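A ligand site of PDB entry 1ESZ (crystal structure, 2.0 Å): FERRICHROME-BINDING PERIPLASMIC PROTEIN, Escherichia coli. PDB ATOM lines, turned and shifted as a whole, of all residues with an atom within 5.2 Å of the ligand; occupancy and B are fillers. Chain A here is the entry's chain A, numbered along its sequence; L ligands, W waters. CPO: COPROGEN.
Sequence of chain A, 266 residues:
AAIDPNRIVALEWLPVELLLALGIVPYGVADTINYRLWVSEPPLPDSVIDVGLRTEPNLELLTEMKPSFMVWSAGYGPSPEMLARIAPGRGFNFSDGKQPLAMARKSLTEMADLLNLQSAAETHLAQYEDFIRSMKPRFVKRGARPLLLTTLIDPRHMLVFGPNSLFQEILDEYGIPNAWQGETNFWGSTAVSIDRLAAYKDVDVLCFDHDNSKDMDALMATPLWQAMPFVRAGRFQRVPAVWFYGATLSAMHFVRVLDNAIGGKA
An oxygen (O5) of the ligand sits at hydrogen-bond distance from the side-chain hydroxyl (OG) of Ser 73, 3.0 Å away.
The side-chain hydroxyl of Tyr 76 lies close to an oxygen (O7) of the ligand, 2.6 Å away.
OD1 of Asn 185 sits at hydrogen-bond distance from N of Trp 187.
The guanidinium group (NE) of Arg 54 is in salt-bridge range of the side-chain carboxylate (OE2) of Glu 12 (3.1 Å).
OH of Tyr 76 is in hydrogen-bond range of NH2 of Arg 54 (3.4 Å).
OE1 of Glu 12 lies within hydrogen-bond range of OG of Ser 73, at 2.6 Å.
The side-chain carboxylate (OD2) of Asp 31 lies within hydrogen-bond range of the side-chain amide nitrogen (ND2) of Asn 34 (2.8 Å).
OE1 of Glu 12 sits at hydrogen-bond distance from N of Leu 14, at 3.0 Å.
The backbone NH (N) of Trp 243 is in hydrogen-bond range of the backbone carbonyl oxygen (O) of Trp 38, at 3.5 Å.
The guanidinium group (NH2) of Arg 54 sits close to an oxygen (O12) of the ligand.
Merely in contact with the ligand: Glu 12, Trp 38, Trp 187, Tyr 245, Phe 94, Trp 243, Ile 153, Phe 244, Leu 14, Thr 55 and Asn 34.
Hydrophobic or aromatic side chains within 4 Å of the ligand: Leu 14, Trp 38, Tyr 76, Phe 94, Ile 153, Trp 187, Trp 243, Phe 244 and Tyr 245.
Of the 20 residues printed, 14 come within 4 Å of the ligand.
Along chain A the residues within 4 Å of the ligand span positions 12 to 245.
The nearest printed residue that does not touch the ligand is Leu 159 (4.1 Å).
Water W2 lies within hydrogen-bond range of OH of Tyr 245 (2.6 Å) and O13 of the ligand (3.1 Å).
Water W3 lies within hydrogen-bond range of the backbone carbonyl oxygen (O) of Ala 74 (2.9 Å), the indole nitrogen (NE1) of Trp 187 (2.9 Å) and an oxygen (O5) of the ligand (3.0 Å).
Water W4 bridges OD1 of Asn 34 and NE1 of Trp 38.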
ATOM      1  N   GLU A  12     -18.849 -28.885 -15.248  1.00  0.00           N
ATOM      2  CA  GLU A  12     -19.741 -28.826 -16.394  1.00  0.00           C
ATOM      3  C   GLU A  12     -21.148 -28.907 -15.823  1.00  0.00           C
ATOM      4  O   GLU A  12     -21.356 -29.466 -14.745  1.00  0.00           O
ATOM      5  CB  GLU A  12     -19.433 -29.980 -17.353  1.00  0.00           C
ATOM      6  CG  GLU A  12     -19.747 -29.662 -18.812  1.00  0.00           C
ATOM      7  CD  GLU A  12     -21.224 -29.463 -19.042  1.00  0.00           C
ATOM      8  OE1 GLU A  12     -21.961 -30.465 -18.919  1.00  0.00           O
ATOM      9  OE2 GLU A  12     -21.648 -28.320 -19.333  1.00  0.00           O
ATOM     10  N   TRP A  13     -22.124 -28.351 -16.536  1.00  0.00           N
ATOM     11  CA  TRP A  13     -23.486 -28.316 -16.027  1.00  0.00           C
ATOM     12  C   TRP A  13     -24.259 -29.635 -15.917  1.00  0.00           C
ATOM     13  O   TRP A  13     -25.211 -29.718 -15.145  1.00  0.00           O
ATOM     14  CB  TRP A  13     -24.318 -27.306 -16.828  1.00  0.00           C
ATOM     15  CG  TRP A  13     -23.711 -25.922 -16.850  1.00  0.00           C
ATOM     16  CD1 TRP A  13     -22.856 -25.369 -15.929  1.00  0.00           C
ATOM     17  CD2 TRP A  13     -23.909 -24.927 -17.861  1.00  0.00           C
ATOM     18  NE1 TRP A  13     -22.507 -24.101 -16.306  1.00  0.00           N
ATOM     19  CE2 TRP A  13     -23.140 -23.793 -17.489  1.00  0.00           C
ATOM     20  CE3 TRP A  13     -24.656 -24.871 -19.045  1.00  0.00           C
ATOM     21  CZ2 TRP A  13     -23.092 -22.621 -18.266  1.00  0.00           C
ATOM     22  CZ3 TRP A  13     -24.614 -23.704 -19.815  1.00  0.00           C
ATOM     23  CH2 TRP A  13     -23.833 -22.597 -19.424  1.00  0.00           C
ATOM     24  N   LEU A  14     -23.865 -30.663 -16.674  1.00  0.00           N
ATOM     25  CA  LEU A  14     -24.568 -31.947 -16.577  1.00  0.00           C
ATOM     26  C   LEU A  14     -24.458 -32.507 -15.146  1.00  0.00           C
ATOM     27  O   LEU A  14     -25.466 -32.776 -14.496  1.00  0.00           O
ATOM     28  CB  LEU A  14     -23.995 -32.949 -17.601  1.00  0.00           C
ATOM     29  CG  LEU A  14     -24.411 -34.418 -17.473  1.00  0.00           C
ATOM     30  CD1 LEU A  14     -25.929 -34.538 -17.584  1.00  0.00           C
ATOM     31  CD2 LEU A  14     -23.738 -35.255 -18.587  1.00  0.00           C
ATOM     32  N   ASP A  31     -18.783 -21.481 -14.568  1.00  0.00           N
ATOM     33  CA  ASP A  31     -19.697 -20.569 -15.268  1.00  0.00           C
ATOM     34  C   ASP A  31     -21.111 -20.520 -14.664  1.00  0.00           C
ATOM     35  O   ASP A  31     -22.093 -20.887 -15.315  1.00  0.00           O
ATOM     36  CB  ASP A  31     -19.760 -20.966 -16.756  1.00  0.00           C
ATOM     37  CG  ASP A  31     -20.353 -19.871 -17.640  1.00  0.00           C
ATOM     38  OD1 ASP A  31     -20.426 -20.079 -18.871  1.00  0.00           O
ATOM     39  OD2 ASP A  31     -20.741 -18.813 -17.105  1.00  0.00           O
ATOM     40  N   ASN A  34     -23.751 -18.095 -16.677  1.00  0.00           N
ATOM     41  CA  ASN A  34     -24.501 -18.680 -17.775  1.00  0.00           C
ATOM     42  C   ASN A  34     -25.332 -19.880 -17.376  1.00  0.00           C
ATOM     43  O   ASN A  34     -26.297 -20.219 -18.053  1.00  0.00           O
ATOM     44  CB  ASN A  34     -23.544 -19.008 -18.915  1.00  0.00           C
ATOM     45  CG  ASN A  34     -22.959 -17.742 -19.538  1.00  0.00           C
ATOM     46  OD1 ASN A  34     -23.696 -16.903 -20.038  1.00  0.00           O
ATOM     47  ND2 ASN A  34     -21.640 -17.613 -19.489  1.00  0.00           N
ATOM     48  N   TRP A  38     -28.971 -20.276 -18.879  1.00  0.00           N
ATOM     49  CA  TRP A  38     -29.158 -21.343 -19.868  1.00  0.00           C
ATOM     50  C   TRP A  38     -29.859 -22.549 -19.248  1.00  0.00           C
ATOM     51  O   TRP A  38     -30.635 -23.245 -19.916  1.00  0.00           O
ATOM     52  CB  TRP A  38     -27.819 -21.793 -20.467  1.00  0.00           C
ATOM     53  CG  TRP A  38     -27.256 -20.831 -21.465  1.00  0.00           C
ATOM     54  CD1 TRP A  38     -26.425 -19.777 -21.206  1.00  0.00           C
ATOM     55  CD2 TRP A  38     -27.476 -20.842 -22.882  1.00  0.00           C
ATOM     56  NE1 TRP A  38     -26.118 -19.122 -22.375  1.00  0.00           N
ATOM     57  CE2 TRP A  38     -26.741 -19.754 -23.414  1.00  0.00           C
ATOM     58  CE3 TRP A  38     -28.211 -21.658 -23.743  1.00  0.00           C
ATOM     59  CZ2 TRP A  38     -26.727 -19.466 -24.789  1.00  0.00           C
ATOM     60  CZ3 TRP A  38     -28.205 -21.365 -25.106  1.00  0.00           C
ATOM     61  CH2 TRP A  38     -27.465 -20.278 -25.609  1.00  0.00           C
ATOM     62  N   ARG A  54     -16.422 -23.450 -18.323  1.00  0.00           N
ATOM     63  CA  ARG A  54     -16.344 -24.904 -18.429  1.00  0.00           C
ATOM     64  C   ARG A  54     -15.231 -25.309 -19.372  1.00  0.00           C
ATOM     65  O   ARG A  54     -14.610 -26.344 -19.192  1.00  0.00           O
ATOM     66  CB  ARG A  54     -17.674 -25.479 -18.930  1.00  0.00           C
ATOM     67  CG  ARG A  54     -18.859 -25.117 -18.061  1.00  0.00           C
ATOM     68  CD  ARG A  54     -19.916 -24.428 -18.898  1.00  0.00           C
ATOM     69  NE  ARG A  54     -20.641 -25.379 -19.725  1.00  0.00           N
ATOM     70  CZ  ARG A  54     -21.157 -25.113 -20.921  1.00  0.00           C
ATOM     71  NH1 ARG A  54     -21.026 -23.923 -21.482  1.00  0.00           N
ATOM     72  NH2 ARG A  54     -21.832 -26.067 -21.554  1.00  0.00           N
ATOM     73  N   THR A  55     -14.988 -24.479 -20.384  1.00  0.00           N
ATOM     74  CA  THR A  55     -13.957 -24.762 -21.379  1.00  0.00           C
ATOM     75  C   THR A  55     -12.568 -24.298 -20.972  1.00  0.00           C
ATOM     76  O   THR A  55     -11.588 -24.628 -21.623  1.00  0.00           O
ATOM     77  CB  THR A  55     -14.302 -24.108 -22.725  1.00  0.00           C
ATOM     78  OG1 THR A  55     -14.513 -22.711 -22.513  1.00  0.00           O
ATOM     79  CG2 THR A  55     -15.565 -24.720 -23.310  1.00  0.00           C
ATOM     80  N   SER A  73     -18.157 -33.441 -17.768  1.00  0.00           N
ATOM     81  CA  SER A  73     -18.779 -34.154 -18.882  1.00  0.00           C
ATOM     82  C   SER A  73     -17.738 -34.827 -19.766  1.00  0.00           C
ATOM     83  O   SER A  73     -16.736 -34.208 -20.141  1.00  0.00           O
ATOM     84  CB  SER A  73     -19.624 -33.201 -19.739  1.00  0.00           C
ATOM     85  OG  SER A  73     -20.819 -32.826 -19.087  1.00  0.00           O
ATOM     86  N   ALA A  74     -17.995 -36.083 -20.118  1.00  0.00           N
ATOM     87  CA  ALA A  74     -17.108 -36.884 -20.955  1.00  0.00           C
ATOM     88  C   ALA A  74     -16.829 -36.216 -22.298  1.00  0.00           C
ATOM     89  O   ALA A  74     -17.740 -35.751 -22.967  1.00  0.00           O
ATOM     90  CB  ALA A  74     -17.733 -38.268 -21.176  1.00  0.00           C
ATOM     91  N   TYR A  76     -15.636 -33.419 -22.974  1.00  0.00           N
ATOM     92  CA  TYR A  76     -15.873 -31.964 -22.990  1.00  0.00           C
ATOM     93  C   TYR A  76     -14.959 -31.270 -21.971  1.00  0.00           C
ATOM     94  O   TYR A  76     -14.767 -31.752 -20.857  1.00  0.00           O
ATOM     95  CB  TYR A  76     -17.340 -31.666 -22.638  1.00  0.00           C
ATOM     96  CG  TYR A  76     -17.759 -30.219 -22.851  1.00  0.00           C
ATOM     97  CD1 TYR A  76     -18.348 -29.822 -24.058  1.00  0.00           C
ATOM     98  CD2 TYR A  76     -17.577 -29.254 -21.859  1.00  0.00           C
ATOM     99  CE1 TYR A  76     -18.742 -28.496 -24.260  1.00  0.00           C
ATOM    100  CE2 TYR A  76     -17.964 -27.920 -22.051  1.00  0.00           C
ATOM    101  CZ  TYR A  76     -18.552 -27.554 -23.263  1.00  0.00           C
ATOM    102  OH  TYR A  76     -18.975 -26.251 -23.457  1.00  0.00           O
ATOM    103  N   PHE A  92     -18.856 -37.730 -16.597  1.00  0.00           N
ATOM    104  CA  PHE A  92     -20.127 -38.386 -16.848  1.00  0.00           C
ATOM    105  C   PHE A  92     -20.529 -38.289 -18.312  1.00  0.00           C
ATOM    106  O   PHE A  92     -20.231 -37.299 -18.986  1.00  0.00           O
ATOM    107  CB  PHE A  92     -21.234 -37.810 -15.960  1.00  0.00           C
ATOM    108  CG  PHE A  92     -21.060 -38.162 -14.508  1.00  0.00           C
ATOM    109  CD1 PHE A  92     -20.098 -37.533 -13.726  1.00  0.00           C
ATOM    110  CD2 PHE A  92     -21.830 -39.172 -13.940  1.00  0.00           C
ATOM    111  CE1 PHE A  92     -19.888 -37.910 -12.401  1.00  0.00           C
ATOM    112  CE2 PHE A  92     -21.623 -39.563 -12.611  1.00  0.00           C
ATOM    113  CZ  PHE A  92     -20.650 -38.925 -11.843  1.00  0.00           C
ATOM    114  N   PHE A  94     -23.242 -37.971 -21.349  1.00  0.00           N
ATOM    115  CA  PHE A  94     -24.522 -37.343 -21.604  1.00  0.00           C
ATOM    116  C   PHE A  94     -25.434 -38.336 -22.314  1.00  0.00           C
ATOM    117  O   PHE A  94     -26.645 -38.327 -22.123  1.00  0.00           O
ATOM    118  CB  PHE A  94     -24.370 -36.128 -22.500  1.00  0.00           C
ATOM    119  CG  PHE A  94     -25.665 -35.630 -23.061  1.00  0.00           C
ATOM    120  CD1 PHE A  94     -26.628 -35.078 -22.210  1.00  0.00           C
ATOM    121  CD2 PHE A  94     -25.948 -35.724 -24.423  1.00  0.00           C
ATOM    122  CE1 PHE A  94     -27.844 -34.641 -22.712  1.00  0.00           C
ATOM    123  CE2 PHE A  94     -27.175 -35.278 -24.927  1.00  0.00           C
ATOM    124  CZ  PHE A  94     -28.119 -34.736 -24.069  1.00  0.00           C
ATOM    125  N   ILE A 153     -28.702 -19.232 -32.260  1.00  0.00           N
ATOM    126  CA  ILE A 153     -27.298 -19.099 -31.907  1.00  0.00           C
ATOM    127  C   ILE A 153     -26.861 -17.664 -32.231  1.00  0.00           C
ATOM    128  O   ILE A 153     -26.238 -16.988 -31.424  1.00  0.00           O
ATOM    129  CB  ILE A 153     -26.432 -20.078 -32.703  1.00  0.00           C
ATOM    130  CG1 ILE A 153     -26.890 -21.513 -32.421  1.00  0.00           C
ATOM    131  CG2 ILE A 153     -24.966 -19.911 -32.315  1.00  0.00           C
ATOM    132  CD1 ILE A 153     -26.175 -22.555 -33.264  1.00  0.00           C
ATOM    133  N   LEU A 159     -30.005 -23.530 -33.893  1.00  0.00           N
ATOM    134  CA  LEU A 159     -29.712 -24.879 -33.435  1.00  0.00           C
ATOM    135  C   LEU A 159     -31.044 -25.617 -33.453  1.00  0.00           C
ATOM    136  O   LEU A 159     -32.067 -25.068 -33.052  1.00  0.00           O
ATOM    137  CB  LEU A 159     -29.160 -24.875 -32.011  1.00  0.00           C
ATOM    138  CG  LEU A 159     -27.697 -25.266 -31.785  1.00  0.00           C
ATOM    139  CD1 LEU A 159     -27.443 -25.373 -30.281  1.00  0.00           C
ATOM    140  CD2 LEU A 159     -27.399 -26.597 -32.466  1.00  0.00           C
ATOM    141  N   ASN A 185     -25.383 -34.012 -34.190  1.00  0.00           N
ATOM    142  CA  ASN A 185     -24.086 -34.300 -33.623  1.00  0.00           C
ATOM    143  C   ASN A 185     -24.365 -35.327 -32.511  1.00  0.00           C
ATOM    144  O   ASN A 185     -25.504 -35.758 -32.320  1.00  0.00           O
ATOM    145  CB  ASN A 185     -23.421 -33.032 -33.052  1.00  0.00           C
ATOM    146  CG  ASN A 185     -24.315 -32.292 -32.080  1.00  0.00           C
ATOM    147  OD1 ASN A 185     -25.086 -32.888 -31.331  1.00  0.00           O
ATOM    148  ND2 ASN A 185     -24.202 -30.961 -32.067  1.00  0.00           N
ATOM    149  N   TRP A 187     -24.538 -35.007 -29.361  1.00  0.00           N
ATOM    150  CA  TRP A 187     -25.475 -34.516 -28.354  1.00  0.00           C
ATOM    151  C   TRP A 187     -26.900 -34.263 -28.839  1.00  0.00           C
ATOM    152  O   TRP A 187     -27.724 -33.745 -28.090  1.00  0.00           O
ATOM    153  CB  TRP A 187     -24.885 -33.265 -27.708  1.00  0.00           C
ATOM    154  CG  TRP A 187     -23.504 -33.515 -27.156  1.00  0.00           C
ATOM    155  CD1 TRP A 187     -23.180 -33.925 -25.894  1.00  0.00           C
ATOM    156  CD2 TRP A 187     -22.277 -33.455 -27.890  1.00  0.00           C
ATOM    157  NE1 TRP A 187     -21.817 -34.128 -25.800  1.00  0.00           N
ATOM    158  CE2 TRP A 187     -21.241 -33.844 -27.008  1.00  0.00           C
ATOM    159  CE3 TRP A 187     -21.936 -33.116 -29.212  1.00  0.00           C
ATOM    160  CZ2 TRP A 187     -19.900 -33.903 -27.396  1.00  0.00           C
ATOM    161  CZ3 TRP A 187     -20.608 -33.178 -29.599  1.00  0.00           C
ATOM    162  CH2 TRP A 187     -19.599 -33.572 -28.697  1.00  0.00           C
ATOM    163  N   TRP A 243     -32.126 -26.312 -20.514  1.00  0.00           N
ATOM    164  CA  TRP A 243     -30.826 -26.835 -20.914  1.00  0.00           C
ATOM    165  C   TRP A 243     -31.012 -28.124 -21.697  1.00  0.00           C
ATOM    166  O   TRP A 243     -31.559 -29.085 -21.190  1.00  0.00           O
ATOM    167  CB  TRP A 243     -29.963 -27.095 -19.679  1.00  0.00           C
ATOM    168  CG  TRP A 243     -28.528 -27.429 -20.021  1.00  0.00           C
ATOM    169  CD1 TRP A 243     -27.755 -28.400 -19.453  1.00  0.00           C
ATOM    170  CD2 TRP A 243     -27.707 -26.786 -21.006  1.00  0.00           C
ATOM    171  NE1 TRP A 243     -26.502 -28.396 -20.014  1.00  0.00           N
ATOM    172  CE2 TRP A 243     -26.448 -27.416 -20.970  1.00  0.00           C
ATOM    173  CE3 TRP A 243     -27.916 -25.729 -21.907  1.00  0.00           C
ATOM    174  CZ2 TRP A 243     -25.397 -27.034 -21.806  1.00  0.00           C
ATOM    175  CZ3 TRP A 243     -26.878 -25.351 -22.741  1.00  0.00           C
ATOM    176  CH2 TRP A 243     -25.628 -25.999 -22.695  1.00  0.00           C
ATOM    177  N   PHE A 244     -30.522 -28.151 -22.935  1.00  0.00           N
ATOM    178  CA  PHE A 244     -30.690 -29.332 -23.777  1.00  0.00           C
ATOM    179  C   PHE A 244     -29.648 -30.442 -23.637  1.00  0.00           C
ATOM    180  O   PHE A 244     -29.801 -31.515 -24.226  1.00  0.00           O
ATOM    181  CB  PHE A 244     -30.804 -28.893 -25.242  1.00  0.00           C
ATOM    182  CG  PHE A 244     -30.203 -27.551 -25.510  1.00  0.00           C
ATOM    183  CD1 PHE A 244     -28.858 -27.414 -25.805  1.00  0.00           C
ATOM    184  CD2 PHE A 244     -30.996 -26.408 -25.445  1.00  0.00           C
ATOM    185  CE1 PHE A 244     -28.294 -26.152 -26.038  1.00  0.00           C
ATOM    186  CE2 PHE A 244     -30.445 -25.151 -25.677  1.00  0.00           C
ATOM    187  CZ  PHE A 244     -29.098 -25.023 -25.976  1.00  0.00           C
ATOM    188  N   TYR A 245     -28.612 -30.186 -22.853  1.00  0.00           N
ATOM    189  CA  TYR A 245     -27.564 -31.167 -22.645  1.00  0.00           C
ATOM    190  C   TYR A 245     -27.529 -31.588 -21.168  1.00  0.00           C
ATOM    191  O   TYR A 245     -26.474 -31.982 -20.655  1.00  0.00           O
ATOM    192  CB  TYR A 245     -26.212 -30.590 -23.076  1.00  0.00           C
ATOM    193  CG  TYR A 245     -26.200 -30.086 -24.511  1.00  0.00           C
ATOM    194  CD1 TYR A 245     -25.507 -28.924 -24.851  1.00  0.00           C
ATOM    195  CD2 TYR A 245     -26.883 -30.772 -25.516  1.00  0.00           C
ATOM    196  CE1 TYR A 245     -25.490 -28.458 -26.170  1.00  0.00           C
ATOM    197  CE2 TYR A 245     -26.864 -30.314 -26.838  1.00  0.00           C
ATOM    198  CZ  TYR A 245     -26.175 -29.153 -27.154  1.00  0.00           C
ATOM    199  OH  TYR A 245     -26.160 -28.695 -28.452  1.00  0.00           O
HETATM  200  C1  CPO L   1     -18.445 -28.876 -30.205  1.00  0.00           C
HETATM  201  C2  CPO L   1     -18.292 -30.005 -29.169  1.00  0.00           C
HETATM  202  C3  CPO L   1     -19.626 -30.265 -28.372  1.00  0.00           C
HETATM  203  C4  CPO L   1     -20.966 -29.478 -28.640  1.00  0.00           C
HETATM  204  C5  CPO L   1     -22.126 -29.645 -27.668  1.00  0.00           C
HETATM  205  N1  CPO L   1     -22.194 -28.477 -26.833  1.00  0.00           N
HETATM  206  C6  CPO L   1     -22.103 -28.579 -25.518  1.00  0.00           C
HETATM  207  O1  CPO L   1     -19.198 -29.011 -31.155  1.00  0.00           O
HETATM  208  N2  CPO L   1     -17.371 -29.705 -28.140  1.00  0.00           N
HETATM  209  O2  CPO L   1     -22.356 -27.255 -27.385  1.00  0.00           O
HETATM  210  O3  CPO L   1     -22.153 -27.584 -24.843  1.00  0.00           O
HETATM  211  C7  CPO L   1     -16.655 -28.540 -27.975  1.00  0.00           C
HETATM  212  C8  CPO L   1     -16.827 -27.361 -29.035  1.00  0.00           C
HETATM  213  C9  CPO L   1     -17.718 -26.463 -28.169  1.00  0.00           C
HETATM  214  C10 CPO L   1     -17.146 -25.449 -27.164  1.00  0.00           C
HETATM  215  C11 CPO L   1     -18.159 -24.678 -26.283  1.00  0.00           C
HETATM  216  O4  CPO L   1     -15.879 -28.374 -27.058  1.00  0.00           O
HETATM  217  N3  CPO L   1     -17.732 -27.707 -30.053  1.00  0.00           N
HETATM  218  C12 CPO L   1     -21.756 -29.155 -22.336  1.00  0.00           C
HETATM  219  C13 CPO L   1     -22.149 -30.248 -23.415  1.00  0.00           C
HETATM  220  C14 CPO L   1     -22.804 -31.591 -22.941  1.00  0.00           C
HETATM  221  C15 CPO L   1     -21.667 -32.435 -22.373  1.00  0.00           C
HETATM  222  O5  CPO L   1     -22.220 -33.465 -21.680  1.00  0.00           O
HETATM  223  C16 CPO L   1     -21.903 -30.004 -24.833  1.00  0.00           C
HETATM  224 FE   CPO L   1     -22.143 -25.862 -25.938  1.00  0.00          FE
HETATM  225  N4  CPO L   1     -19.611 -24.920 -26.409  1.00  0.00           N
HETATM  226  C17 CPO L   1     -20.356 -24.157 -27.205  1.00  0.00           C
HETATM  227  C18 CPO L   1     -19.708 -23.002 -28.054  1.00  0.00           C
HETATM  228  C19 CPO L   1     -19.425 -21.765 -27.615  1.00  0.00           C
HETATM  229  C20 CPO L   1     -19.221 -20.639 -28.610  1.00  0.00           C
HETATM  230  C21 CPO L   1     -20.495 -19.740 -28.684  1.00  0.00           C
HETATM  231  O6  CPO L   1     -21.571 -20.539 -29.268  1.00  0.00           O
HETATM  232  O7  CPO L   1     -20.179 -25.887 -25.743  1.00  0.00           O
HETATM  233  O8  CPO L   1     -21.623 -24.394 -27.282  1.00  0.00           O
HETATM  234  C23 CPO L   1     -22.623 -20.686 -28.276  1.00  0.00           C
HETATM  235  C24 CPO L   1     -23.479 -22.002 -28.222  1.00  0.00           C
HETATM  236  C25 CPO L   1     -24.884 -21.774 -27.640  1.00  0.00           C
HETATM  237  C26 CPO L   1     -25.695 -23.075 -27.437  1.00  0.00           C
HETATM  238  C27 CPO L   1     -25.501 -23.637 -26.005  1.00  0.00           C
HETATM  239  N5  CPO L   1     -24.367 -24.344 -25.680  1.00  0.00           N
HETATM  240  C28 CPO L   1     -23.593 -23.946 -24.733  1.00  0.00           C
HETATM  241  C29 CPO L   1     -23.934 -22.606 -23.914  1.00  0.00           C
HETATM  242  C30 CPO L   1     -22.821 -21.538 -23.807  1.00  0.00           C
HETATM  243  C31 CPO L   1     -23.316 -20.021 -23.759  1.00  0.00           C
HETATM  244  C32 CPO L   1     -22.178 -19.126 -23.156  1.00  0.00           C
HETATM  245  O9  CPO L   1     -21.607 -18.342 -24.228  1.00  0.00           O
HETATM  246  O10 CPO L   1     -22.846 -19.765 -27.454  1.00  0.00           O
HETATM  247  O11 CPO L   1     -24.053 -25.479 -26.340  1.00  0.00           O
HETATM  248  O12 CPO L   1     -22.593 -24.600 -24.455  1.00  0.00           O
HETATM  249  C33 CPO L   1     -21.576 -21.838 -24.475  1.00  0.00           C
HETATM  250  N6  CPO L   1     -23.728 -22.299 -29.534  1.00  0.00           N
HETATM  251  C34 CPO L   1     -23.090 -23.170 -30.381  1.00  0.00           C
HETATM  252  O13 CPO L   1     -22.787 -24.353 -29.966  1.00  0.00           O
HETATM  253  C35 CPO L   1     -22.756 -22.740 -31.815  1.00  0.00           C
HETATM  254  O   HOH W   1     -21.137 -27.391 -32.848  1.00  0.00           O
HETATM  255  O   HOH W   2     -24.420 -26.861 -29.159  1.00  0.00           O
HETATM  256  O   HOH W   3     -20.545 -35.273 -23.450  1.00  0.00           O
HETATM  257  O   HOH W   4     -24.154 -16.266 -22.853  1.00  0.00           O
